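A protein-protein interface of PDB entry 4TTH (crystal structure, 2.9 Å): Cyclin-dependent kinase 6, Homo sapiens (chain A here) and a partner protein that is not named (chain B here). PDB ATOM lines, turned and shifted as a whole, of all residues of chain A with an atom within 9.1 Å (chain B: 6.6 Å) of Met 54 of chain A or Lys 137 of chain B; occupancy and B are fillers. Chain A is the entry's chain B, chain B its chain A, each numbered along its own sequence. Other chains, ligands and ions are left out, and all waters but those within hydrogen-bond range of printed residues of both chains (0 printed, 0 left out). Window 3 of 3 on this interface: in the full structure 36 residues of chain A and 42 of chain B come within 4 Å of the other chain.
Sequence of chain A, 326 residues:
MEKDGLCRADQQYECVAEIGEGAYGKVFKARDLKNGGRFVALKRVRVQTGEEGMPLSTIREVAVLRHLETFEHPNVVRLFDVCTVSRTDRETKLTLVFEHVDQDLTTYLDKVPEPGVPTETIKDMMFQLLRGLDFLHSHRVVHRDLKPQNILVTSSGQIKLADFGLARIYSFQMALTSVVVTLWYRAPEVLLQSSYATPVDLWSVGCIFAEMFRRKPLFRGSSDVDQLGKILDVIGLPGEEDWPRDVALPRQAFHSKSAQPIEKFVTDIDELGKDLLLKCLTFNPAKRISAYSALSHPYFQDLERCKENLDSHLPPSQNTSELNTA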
ATOM      1  N   VAL A  45     -30.327   2.141 -28.787  1.00  0.00           N
ATOM      2  CA  VAL A  45     -29.619   3.395 -29.059  1.00  0.00           C
ATOM      3  C   VAL A  45     -28.159   3.365 -28.609  1.00  0.00           C
ATOM      4  O   VAL A  45     -27.872   3.166 -27.429  1.00  0.00           O
ATOM      5  CB  VAL A  45     -30.319   4.587 -28.373  1.00  0.00           C
ATOM      6  CG1 VAL A  45     -29.509   5.857 -28.558  1.00  0.00           C
ATOM      7  CG2 VAL A  45     -31.741   4.758 -28.912  1.00  0.00           C
ATOM      8  N   ARG A  46     -27.238   3.574 -29.546  1.00  0.00           N
ATOM      9  CA  ARG A  46     -25.818   3.476 -29.229  1.00  0.00           C
ATOM     10  C   ARG A  46     -25.280   4.793 -28.677  1.00  0.00           C
ATOM     11  O   ARG A  46     -25.300   5.820 -29.360  1.00  0.00           O
ATOM     12  CB  ARG A  46     -25.019   3.031 -30.453  1.00  0.00           C
ATOM     13  N   VAL A  47     -24.793   4.749 -27.437  1.00  0.00           N
ATOM     14  CA  VAL A  47     -24.359   5.944 -26.711  1.00  0.00           C
ATOM     15  C   VAL A  47     -22.901   6.321 -26.987  1.00  0.00           C
ATOM     16  O   VAL A  47     -22.066   6.316 -26.081  1.00  0.00           O
ATOM     17  CB  VAL A  47     -24.533   5.751 -25.194  1.00  0.00           C
ATOM     18  CG1 VAL A  47     -24.640   7.103 -24.484  1.00  0.00           C
ATOM     19  CG2 VAL A  47     -25.762   4.898 -24.918  1.00  0.00           C
ATOM     20  N   GLU A  52     -20.477  13.284 -22.871  1.00  0.00           N
ATOM     21  CA  GLU A  52     -21.721  14.039 -23.022  1.00  0.00           C
ATOM     22  C   GLU A  52     -22.920  13.439 -22.304  1.00  0.00           C
ATOM     23  O   GLU A  52     -23.920  14.120 -22.095  1.00  0.00           O
ATOM     24  CB  GLU A  52     -22.065  14.229 -24.498  1.00  0.00           C
ATOM     25  CG  GLU A  52     -21.483  15.488 -25.082  1.00  0.00           C
ATOM     26  CD  GLU A  52     -21.903  16.735 -24.311  1.00  0.00           C
ATOM     27  OE1 GLU A  52     -22.907  17.357 -24.710  1.00  0.00           O
ATOM     28  OE2 GLU A  52     -21.232  17.099 -23.314  1.00  0.00           O
ATOM     29  N   GLY A  53     -22.823  12.168 -21.933  1.00  0.00           N
ATOM     30  CA  GLY A  53     -23.946  11.475 -21.340  1.00  0.00           C
ATOM     31  C   GLY A  53     -24.955  11.089 -22.405  1.00  0.00           C
ATOM     32  O   GLY A  53     -24.614  11.026 -23.590  1.00  0.00           O
ATOM     33  N   MET A  54     -26.196  10.846 -21.985  1.00  0.00           N
ATOM     34  CA  MET A  54     -27.223  10.299 -22.874  1.00  0.00           C
ATOM     35  C   MET A  54     -27.553  11.228 -24.028  1.00  0.00           C
ATOM     36  O   MET A  54     -27.731  12.426 -23.819  1.00  0.00           O
ATOM     37  CB  MET A  54     -28.502  10.019 -22.097  1.00  0.00           C
ATOM     38  CG  MET A  54     -28.317   9.177 -20.863  1.00  0.00           C
ATOM     39  SD  MET A  54     -27.788   7.512 -21.243  1.00  0.00           S
ATOM     40  CE  MET A  54     -28.152   6.696 -19.688  1.00  0.00           C
ATOM     41  N   PRO A  55     -27.654  10.670 -25.248  1.00  0.00           N
ATOM     42  CA  PRO A  55     -27.936  11.431 -26.470  1.00  0.00           C
ATOM     43  C   PRO A  55     -29.089  12.395 -26.250  1.00  0.00           C
ATOM     44  O   PRO A  55     -30.105  12.028 -25.647  1.00  0.00           O
ATOM     45  CB  PRO A  55     -28.346  10.352 -27.469  1.00  0.00           C
ATOM     46  CG  PRO A  55     -27.689   9.126 -26.991  1.00  0.00           C
ATOM     47  CD  PRO A  55     -27.584   9.221 -25.500  1.00  0.00           C
ATOM     48  N   LEU A  56     -28.921  13.621 -26.721  1.00  0.00           N
ATOM     49  CA  LEU A  56     -29.882  14.686 -26.480  1.00  0.00           C
ATOM     50  C   LEU A  56     -31.249  14.245 -26.953  1.00  0.00           C
ATOM     51  O   LEU A  56     -32.249  14.478 -26.287  1.00  0.00           O
ATOM     52  CB  LEU A  56     -29.438  15.940 -27.236  1.00  0.00           C
ATOM     53  CG  LEU A  56     -30.173  17.276 -27.162  1.00  0.00           C
ATOM     54  CD1 LEU A  56     -29.224  18.350 -27.600  1.00  0.00           C
ATOM     55  CD2 LEU A  56     -31.388  17.305 -28.066  1.00  0.00           C
ATOM     56  N   SER A  57     -31.274  13.576 -28.099  1.00  0.00           N
ATOM     57  CA  SER A  57     -32.508  13.342 -28.823  1.00  0.00           C
ATOM     58  C   SER A  57     -33.362  12.287 -28.178  1.00  0.00           C
ATOM     59  O   SER A  57     -34.576  12.453 -28.075  1.00  0.00           O
ATOM     60  CB  SER A  57     -32.228  12.944 -30.258  1.00  0.00           C
ATOM     61  OG  SER A  57     -33.363  13.212 -31.050  1.00  0.00           O
ATOM     62  N   THR A  58     -32.752  11.192 -27.751  1.00  0.00           N
ATOM     63  CA  THR A  58     -33.554  10.163 -27.106  1.00  0.00           C
ATOM     64  C   THR A  58     -34.106  10.666 -25.789  1.00  0.00           C
ATOM     65  O   THR A  58     -35.213  10.325 -25.433  1.00  0.00           O
ATOM     66  CB  THR A  58     -32.803   8.841 -26.883  1.00  0.00           C
ATOM     67  OG1 THR A  58     -31.598   9.090 -26.150  1.00  0.00           O
ATOM     68  CG2 THR A  58     -32.480   8.169 -28.218  1.00  0.00           C
ATOM     69  N   ILE A  59     -33.347  11.485 -25.073  1.00  0.00           N
ATOM     70  CA  ILE A  59     -33.846  12.060 -23.829  1.00  0.00           C
ATOM     71  C   ILE A  59     -35.065  12.930 -24.097  1.00  0.00           C
ATOM     72  O   ILE A  59     -36.027  12.901 -23.345  1.00  0.00           O
ATOM     73  CB  ILE A  59     -32.766  12.881 -23.093  1.00  0.00           C
ATOM     74  CG1 ILE A  59     -31.727  11.953 -22.466  1.00  0.00           C
ATOM     75  CG2 ILE A  59     -33.388  13.757 -22.008  1.00  0.00           C
ATOM     76  CD1 ILE A  59     -30.778  12.664 -21.532  1.00  0.00           C
ATOM     77  N   ARG A  60     -35.029  13.691 -25.181  1.00  0.00           N
ATOM     78  CA  ARG A  60     -36.192  14.454 -25.615  1.00  0.00           C
ATOM     79  C   ARG A  60     -37.369  13.557 -25.984  1.00  0.00           C
ATOM     80  O   ARG A  60     -38.481  13.752 -25.496  1.00  0.00           O
ATOM     81  CB  ARG A  60     -35.840  15.303 -26.825  1.00  0.00           C
ATOM     82  CG  ARG A  60     -35.195  16.599 -26.473  1.00  0.00           C
ATOM     83  CD  ARG A  60     -35.000  17.444 -27.715  1.00  0.00           C
ATOM     84  NE  ARG A  60     -34.637  18.812 -27.367  1.00  0.00           N
ATOM     85  CZ  ARG A  60     -33.954  19.619 -28.161  1.00  0.00           C
ATOM     86  NH1 ARG A  60     -33.565  19.196 -29.359  1.00  0.00           N
ATOM     87  NH2 ARG A  60     -33.678  20.854 -27.764  1.00  0.00           N
ATOM     88  N   VAL A  62     -38.210  10.299 -25.309  1.00  0.00           N
ATOM     89  CA  VAL A  62     -38.807   9.642 -24.154  1.00  0.00           C
ATOM     90  C   VAL A  62     -39.516  10.606 -23.223  1.00  0.00           C
ATOM     91  O   VAL A  62     -40.594  10.308 -22.714  1.00  0.00           O
ATOM     92  CB  VAL A  62     -37.740   8.964 -23.317  1.00  0.00           C
ATOM     93  CG1 VAL A  62     -38.354   8.363 -22.068  1.00  0.00           C
ATOM     94  CG2 VAL A  62     -37.020   7.922 -24.130  1.00  0.00           C
ATOM     95  N   VAL A  82     -36.816   1.490 -20.492  1.00  0.00           N
ATOM     96  CA  VAL A  82     -35.468   1.881 -20.876  1.00  0.00           C
ATOM     97  C   VAL A  82     -34.495   1.126 -19.962  1.00  0.00           C
ATOM     98  O   VAL A  82     -34.854   0.742 -18.849  1.00  0.00           O
ATOM     99  CB  VAL A  82     -35.250   3.428 -20.770  1.00  0.00           C
ATOM    100  CG1 VAL A  82     -33.924   3.846 -21.402  1.00  0.00           C
ATOM    101  CG2 VAL A  82     -36.377   4.185 -21.437  1.00  0.00           C
ATOM    102  N   CYS A  83     -33.279   0.888 -20.445  1.00  0.00           N
ATOM    103  CA  CYS A  83     -32.243   0.220 -19.655  1.00  0.00           C
ATOM    104  C   CYS A  83     -30.837   0.388 -20.256  1.00  0.00           C
ATOM    105  O   CYS A  83     -30.680   0.556 -21.473  1.00  0.00           O
ATOM    106  CB  CYS A  83     -32.587  -1.260 -19.467  1.00  0.00           C
ATOM    107  SG  CYS A  83     -33.658  -1.938 -20.764  1.00  0.00           S
ATOM    108  N   THR A  84     -29.820   0.343 -19.394  1.00  0.00           N
ATOM    109  CA  THR A  84     -28.435   0.572 -19.810  1.00  0.00           C
ATOM    110  C   THR A  84     -27.558  -0.664 -19.606  1.00  0.00           C
ATOM    111  O   THR A  84     -26.434  -0.567 -19.106  1.00  0.00           O
ATOM    112  CB  THR A  84     -27.794   1.751 -19.042  1.00  0.00           C
ATOM    113  OG1 THR A  84     -27.469   1.340 -17.706  1.00  0.00           O
ATOM    114  CG2 THR A  84     -28.740   2.945 -18.997  1.00  0.00           C
ATOM    115  N   THR A  92     -20.677   1.573 -23.426  1.00  0.00           N
ATOM    116  CA  THR A  92     -21.822   0.814 -22.917  1.00  0.00           C
ATOM    117  C   THR A  92     -23.108   1.124 -23.704  1.00  0.00           C
ATOM    118  O   THR A  92     -23.216   2.186 -24.318  1.00  0.00           O
ATOM    119  CB  THR A  92     -22.021   1.043 -21.402  1.00  0.00           C
ATOM    120  OG1 THR A  92     -21.782   2.423 -21.091  1.00  0.00           O
ATOM    121  CG2 THR A  92     -21.051   0.174 -20.598  1.00  0.00           C
ATOM    122  N   LYS A  93     -24.070   0.198 -23.696  1.00  0.00           N
ATOM    123  CA  LYS A  93     -25.228   0.289 -24.608  1.00  0.00           C
ATOM    124  C   LYS A  93     -26.600   0.543 -23.956  1.00  0.00           C
ATOM    125  O   LYS A  93     -26.796   0.313 -22.756  1.00  0.00           O
ATOM    126  CB  LYS A  93     -25.302  -0.935 -25.541  1.00  0.00           C
ATOM    127  CG  LYS A  93     -25.902  -2.189 -24.909  1.00  0.00           C
ATOM    128  CD  LYS A  93     -26.140  -3.267 -25.957  1.00  0.00           C
ATOM    129  CE  LYS A  93     -26.881  -2.696 -27.158  1.00  0.00           C
ATOM    130  NZ  LYS A  93     -27.073  -3.714 -28.225  1.00  0.00           N
ATOM    131  N   LEU A  94     -27.543   1.003 -24.778  1.00  0.00           N
ATOM    132  CA  LEU A  94     -28.842   1.483 -24.310  1.00  0.00           C
ATOM    133  C   LEU A  94     -29.989   0.906 -25.133  1.00  0.00           C
ATOM    134  O   LEU A  94     -29.918   0.869 -26.361  1.00  0.00           O
ATOM    135  CB  LEU A  94     -28.882   3.011 -24.391  1.00  0.00           C
ATOM    136  CG  LEU A  94     -30.170   3.753 -24.039  1.00  0.00           C
ATOM    137  CD1 LEU A  94     -30.521   3.536 -22.584  1.00  0.00           C
ATOM    138  CD2 LEU A  94     -30.017   5.235 -24.344  1.00  0.00           C
ATOM    139  N   THR A  95     -31.054   0.477 -24.457  1.00  0.00           N
ATOM    140  CA  THR A  95     -32.181  -0.166 -25.141  1.00  0.00           C
ATOM    141  C   THR A  95     -33.545   0.468 -24.851  1.00  0.00           C
ATOM    142  O   THR A  95     -33.961   0.595 -23.701  1.00  0.00           O
ATOM    143  CB  THR A  95     -32.240  -1.670 -24.845  1.00  0.00           C
ATOM    144  OG1 THR A  95     -30.946  -2.251 -25.074  1.00  0.00           O
ATOM    145  CG2 THR A  95     -33.258  -2.330 -25.750  1.00  0.00           C
ATOM    146  N   ALA B 100     -26.199  17.977 -12.735  1.00  0.00           N
ATOM    147  CA  ALA B 100     -26.778  16.984 -13.630  1.00  0.00           C
ATOM    148  C   ALA B 100     -28.182  17.417 -14.073  1.00  0.00           C
ATOM    149  O   ALA B 100     -28.564  17.229 -15.232  1.00  0.00           O
ATOM    150  CB  ALA B 100     -26.815  15.630 -12.961  1.00  0.00           C
ATOM    151  N   LEU B 103     -27.849  19.708 -16.702  1.00  0.00           N
ATOM    152  CA  LEU B 103     -27.408  18.980 -17.876  1.00  0.00           C
ATOM    153  C   LEU B 103     -28.610  18.375 -18.594  1.00  0.00           C
ATOM    154  O   LEU B 103     -28.751  18.517 -19.812  1.00  0.00           O
ATOM    155  CB  LEU B 103     -26.404  17.893 -17.515  1.00  0.00           C
ATOM    156  CG  LEU B 103     -25.938  17.216 -18.800  1.00  0.00           C
ATOM    157  CD1 LEU B 103     -25.406  18.258 -19.781  1.00  0.00           C
ATOM    158  CD2 LEU B 103     -24.905  16.131 -18.516  1.00  0.00           C
ATOM    159  N   ILE B 104     -29.482  17.716 -17.830  1.00  0.00           N
ATOM    160  CA  ILE B 104     -30.674  17.083 -18.394  1.00  0.00           C
ATOM    161  C   ILE B 104     -31.664  18.120 -18.918  1.00  0.00           C
ATOM    162  O   ILE B 104     -32.126  18.029 -20.049  1.00  0.00           O
ATOM    163  CB  ILE B 104     -31.397  16.187 -17.364  1.00  0.00           C
ATOM    164  CG1 ILE B 104     -30.499  15.048 -16.879  1.00  0.00           C
ATOM    165  CG2 ILE B 104     -32.653  15.609 -17.967  1.00  0.00           C
ATOM    166  CD1 ILE B 104     -31.035  14.369 -15.645  1.00  0.00           C
ATOM    167  N   LYS B 107     -30.845  19.777 -22.249  1.00  0.00           N
ATOM    168  CA  LYS B 107     -30.938  18.873 -23.378  1.00  0.00           C
ATOM    169  C   LYS B 107     -32.361  18.848 -23.868  1.00  0.00           C
ATOM    170  O   LYS B 107     -32.626  18.679 -25.056  1.00  0.00           O
ATOM    171  CB  LYS B 107     -30.478  17.478 -22.960  1.00  0.00           C
ATOM    172  CG  LYS B 107     -28.971  17.391 -22.778  1.00  0.00           C
ATOM    173  CD  LYS B 107     -28.553  16.126 -22.072  1.00  0.00           C
ATOM    174  CE  LYS B 107     -27.222  15.629 -22.601  1.00  0.00           C
ATOM    175  NZ  LYS B 107     -26.726  14.480 -21.802  1.00  0.00           N
ATOM    176  N   LEU B 132     -20.172  12.892 -13.131  1.00  0.00           N
ATOM    177  CA  LEU B 132     -21.323  13.692 -13.510  1.00  0.00           C
ATOM    178  C   LEU B 132     -22.218  12.933 -14.480  1.00  0.00           C
ATOM    179  O   LEU B 132     -23.433  12.935 -14.337  1.00  0.00           O
ATOM    180  CB  LEU B 132     -20.886  15.012 -14.141  1.00  0.00           C
ATOM    181  CG  LEU B 132     -22.036  15.856 -14.711  1.00  0.00           C
ATOM    182  CD1 LEU B 132     -22.914  16.414 -13.598  1.00  0.00           C
ATOM    183  CD2 LEU B 132     -21.542  16.976 -15.617  1.00  0.00           C
ATOM    184  N   ILE B 133     -21.621  12.292 -15.477  1.00  0.00           N
ATOM    185  CA  ILE B 133     -22.404  11.529 -16.441  1.00  0.00           C
ATOM    186  C   ILE B 133     -23.170  10.406 -15.746  1.00  0.00           C
ATOM    187  O   ILE B 133     -24.372  10.240 -15.960  1.00  0.00           O
ATOM    188  CB  ILE B 133     -21.525  10.914 -17.528  1.00  0.00           C
ATOM    189  CG1 ILE B 133     -20.811  12.004 -18.334  1.00  0.00           C
ATOM    190  CG2 ILE B 133     -22.367  10.041 -18.442  1.00  0.00           C
ATOM    191  CD1 ILE B 133     -19.739  11.453 -19.277  1.00  0.00           C
ATOM    192  N   ASN B 134     -22.471   9.640 -14.914  1.00  0.00           N
ATOM    193  CA  ASN B 134     -23.108   8.613 -14.091  1.00  0.00           C
ATOM    194  C   ASN B 134     -24.235   9.173 -13.231  1.00  0.00           C
ATOM    195  O   ASN B 134     -25.167   8.463 -12.861  1.00  0.00           O
ATOM    196  CB  ASN B 134     -22.078   7.931 -13.192  1.00  0.00           C
ATOM    197  CG  ASN B 134     -21.511   6.681 -13.813  1.00  0.00           C
ATOM    198  OD1 ASN B 134     -22.171   6.033 -14.627  1.00  0.00           O
ATOM    199  ND2 ASN B 134     -20.285   6.327 -13.434  1.00  0.00           N
ATOM    200  N   GLN B 135     -24.135  10.453 -12.909  1.00  0.00           N
ATOM    201  CA  GLN B 135     -25.148  11.114 -12.110  1.00  0.00           C
ATOM    202  C   GLN B 135     -26.313  11.567 -12.984  1.00  0.00           C
ATOM    203  O   GLN B 135     -27.413  11.752 -12.492  1.00  0.00           O
ATOM    204  CB  GLN B 135     -24.537  12.296 -11.365  1.00  0.00           C
ATOM    205  CG  GLN B 135     -25.480  13.006 -10.431  1.00  0.00           C
ATOM    206  CD  GLN B 135     -25.949  12.125  -9.292  1.00  0.00           C
ATOM    207  OE1 GLN B 135     -25.372  12.131  -8.204  1.00  0.00           O
ATOM    208  NE2 GLN B 135     -27.013  11.372  -9.533  1.00  0.00           N
ATOM    209  N   GLU B 136     -26.074  11.751 -14.278  1.00  0.00           N
ATOM    210  CA  GLU B 136     -27.166  12.002 -15.208  1.00  0.00           C
ATOM    211  C   GLU B 136     -27.944  10.712 -15.278  1.00  0.00           C
ATOM    212  O   GLU B 136     -29.169  10.714 -15.233  1.00  0.00           O
ATOM    213  CB  GLU B 136     -26.647  12.369 -16.605  1.00  0.00           C
ATOM    214  CG  GLU B 136     -27.740  12.728 -17.616  1.00  0.00           C
ATOM    215  CD  GLU B 136     -27.204  12.956 -19.029  1.00  0.00           C
ATOM    216  OE1 GLU B 136     -26.465  12.086 -19.541  1.00  0.00           O
ATOM    217  OE2 GLU B 136     -27.534  14.002 -19.631  1.00  0.00           O
ATOM    218  N   LYS B 137     -27.206   9.608 -15.378  1.00  0.00           N
ATOM    219  CA  LYS B 137     -27.779   8.267 -15.412  1.00  0.00           C
ATOM    220  C   LYS B 137     -28.679   8.060 -14.207  1.00  0.00           C
ATOM    221  O   LYS B 137     -29.874   7.831 -14.355  1.00  0.00           O
ATOM    222  CB  LYS B 137     -26.665   7.223 -15.397  1.00  0.00           C
ATOM    223  CG  LYS B 137     -26.892   6.046 -16.317  1.00  0.00           C
ATOM    224  CD  LYS B 137     -25.688   5.108 -16.332  1.00  0.00           C
ATOM    225  CE  LYS B 137     -25.562   4.327 -15.027  1.00  0.00           C
ATOM    226  NZ  LYS B 137     -24.610   3.178 -15.130  1.00  0.00           N
ATOM    227  N   ASP B 138     -28.101   8.163 -13.015  1.00  0.00           N
ATOM    228  CA  ASP B 138     -28.841   7.944 -11.776  1.00  0.00           C
ATOM    229  C   ASP B 138     -30.139   8.719 -11.661  1.00  0.00           C
ATOM    230  O   ASP B 138     -31.109   8.212 -11.116  1.00  0.00           O
ATOM    231  CB  ASP B 138     -27.966   8.257 -10.574  1.00  0.00           C
ATOM    232  CG  ASP B 138     -27.045   7.130 -10.242  1.00  0.00           C
ATOM    233  OD1 ASP B 138     -26.950   6.206 -11.077  1.00  0.00           O
ATOM    234  OD2 ASP B 138     -26.429   7.162  -9.155  1.00  0.00           O
ATOM    235  N   ILE B 139     -30.157   9.951 -12.151  1.00  0.00           N
ATOM    236  CA  ILE B 139     -31.380  10.739 -12.114  1.00  0.00           C
ATOM    237  C   ILE B 139     -32.323  10.269 -13.215  1.00  0.00           C
ATOM    238  O   ILE B 139     -33.547  10.356 -13.080  1.00  0.00           O
ATOM    239  CB  ILE B 139     -31.125  12.261 -12.265  1.00  0.00           C
ATOM    240  CG1 ILE B 139     -30.028  12.731 -11.318  1.00  0.00           C
ATOM    241  CG2 ILE B 139     -32.396  13.055 -11.961  1.00  0.00           C
ATOM    242  CD1 ILE B 139     -29.717  14.190 -11.475  1.00  0.00           C
ATOM    243  N   LEU B 140     -31.759   9.771 -14.309  1.00  0.00           N
ATOM    244  CA  LEU B 140     -32.588   9.271 -15.394  1.00  0.00           C
ATOM    245  C   LEU B 140     -33.334   7.996 -14.985  1.00  0.00           C
ATOM    246  O   LEU B 140     -34.545   7.882 -15.199  1.00  0.00           O
ATOM    247  CB  LEU B 140     -31.757   9.069 -16.656  1.00  0.00           C
ATOM    248  CG  LEU B 140     -31.591  10.389 -17.397  1.00  0.00           C
ATOM    249  CD1 LEU B 140     -30.720  10.232 -18.630  1.00  0.00           C
ATOM    250  CD2 LEU B 140     -32.966  10.944 -17.754  1.00  0.00           C
ATOM    251  N   GLU B 141     -32.613   7.054 -14.382  1.00  0.00           N
ATOM    252  CA  GLU B 141     -33.224   5.843 -13.845  1.00  0.00           C
ATOM    253  C   GLU B 141     -34.300   6.214 -12.830  1.00  0.00           C
ATOM    254  O   GLU B 141     -35.475   6.130 -13.132  1.00  0.00           O
ATOM    255  CB  GLU B 141     -32.159   4.930 -13.232  1.00  0.00           C
ATOM    256  CG  GLU B 141     -31.228   4.325 -14.286  1.00  0.00           C
ATOM    257  CD  GLU B 141     -29.871   3.864 -13.743  1.00  0.00           C
ATOM    258  OE1 GLU B 141     -29.579   4.084 -12.542  1.00  0.00           O
ATOM    259  OE2 GLU B 141     -29.090   3.282 -14.536  1.00  0.00           O
ATOM    260  N   ALA B 142     -33.884   6.664 -11.650  1.00  0.00           N
ATOM    261  CA  ALA B 142     -34.779   7.035 -10.551  1.00  0.00           C
ATOM    262  C   ALA B 142     -36.146   7.619 -10.947  1.00  0.00           C
ATOM    263  O   ALA B 142     -37.160   7.339 -10.305  1.00  0.00           O
ATOM    264  CB  ALA B 142     -34.054   7.981  -9.600  1.00  0.00           C
ATOM    265  N   TRP B 145     -37.004   8.059 -16.510  1.00  0.00           N
ATOM    266  CA  TRP B 145     -36.937   8.916 -17.691  1.00  0.00           C
ATOM    267  C   TRP B 145     -38.148   9.801 -17.890  1.00  0.00           C
ATOM    268  O   TRP B 145     -38.313  10.382 -18.957  1.00  0.00           O
ATOM    269  CB  TRP B 145     -36.676   8.100 -18.953  1.00  0.00           C
ATOM    270  CG  TRP B 145     -35.352   7.449 -18.949  1.00  0.00           C
ATOM    271  CD1 TRP B 145     -34.887   6.545 -18.043  1.00  0.00           C
ATOM    272  CD2 TRP B 145     -34.305   7.642 -19.902  1.00  0.00           C
ATOM    273  NE1 TRP B 145     -33.612   6.163 -18.367  1.00  0.00           N
ATOM    274  CE2 TRP B 145     -33.229   6.820 -19.506  1.00  0.00           C
ATOM    275  CE3 TRP B 145     -34.171   8.429 -21.050  1.00  0.00           C
ATOM    276  CZ2 TRP B 145     -32.031   6.764 -20.215  1.00  0.00           C
ATOM    277  CZ3 TRP B 145     -32.984   8.377 -21.754  1.00  0.00           C
ATOM    278  CH2 TRP B 145     -31.926   7.548 -21.334  1.00  0.00           C
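Gly 53 of chain A touches Lys 107 of chain B. Ile 133 of chain B touches Gly 53 of chain A (CG2 to CA, 3.6 Å). Met 54 of chain A touches Leu 140 of chain B (CG to CD1, 3.4 Å). Met 54 of chain A touches Trp 145 of chain B (CE to CZ2, 3.9 Å). Leu 56 of chain A touches Lys 107 of chain B (CG to O, 3.5 Å). Ile 59 of chain A touches Glu 136 of chain B. Ile 59 of chain A touches Leu 140 of chain B. CZ3 of Trp 145 of chain B touches CG1 of Ile 59 of chain A, at 3.9 Å. Val 62 of chain A touches Trp 145 of chain B. Val 82 of chain A touches Trp 145 of chain B.
Met 54 of chain A touches five residues of chain B. Lys 137 of chain B touches just one residue of chain A: Met 54. Printed residues of chain B within 4 Å of Val 62 of chain A: Trp 145. Of the printed residues of chain B, Val 82 of chain A touches Trp 145 (3.6 Å). Asn 134 of chain B touches none of the printed residues of chain A. Leu 94 of chain A touches none of the printed residues of chain B. The nearest residue of chain B that does not touch Met 54 of chain A is Ile 133 of chain B (5.3 Å). The nearest printed residue of chain A that does not touch Glu 136 of chain B is Glu 52 of chain A (4.1 Å).
The side-chain amino group (NZ) of Lys 107 of chain B lies within salt-bridge range of the side-chain carboxylate (OE1) of Glu 136 of chain B, 3.3 Å away. O of Leu 140 of chain B is in hydrogen-bond range of N of Trp 145 of chain B.
Hydrophobic or aromatic side chains of chain A within 4 Å of the printed part of chain B: Met 54, Leu 56, Ile 59, Val 62 and Val 82. Of the 16 printed residues of chain B, 6 touch a printed residue of chain A. Hydrophobic or aromatic side chains of chain B within 4 Å of the printed part of chain A: Ile 133, Leu 140 and Trp 145. Along chain B the printed residues that touch a printed residue of chain A span positions 107 to 145. Among the printed residues, 16 pairs touch across the chains.
NZ of Lys 107 of chain B sits at hydrogen-bond distance from O of Glu 52 of chain A, at 2.8 Å. NZ of Lys 107 of chain B sits at hydrogen-bond distance from O of Met 54 of chain A, 3.0 Å away. The guanidinium group (NE) of Arg 60 of chain A sits at hydrogen-bond distance from the backbone carbonyl oxygen (O) of Lys 107 of chain B (3.1 Å). N of Met 54 of chain A is in hydrogen-bond range of OE1 of Glu 136 of chain B, at 2.8 Å.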
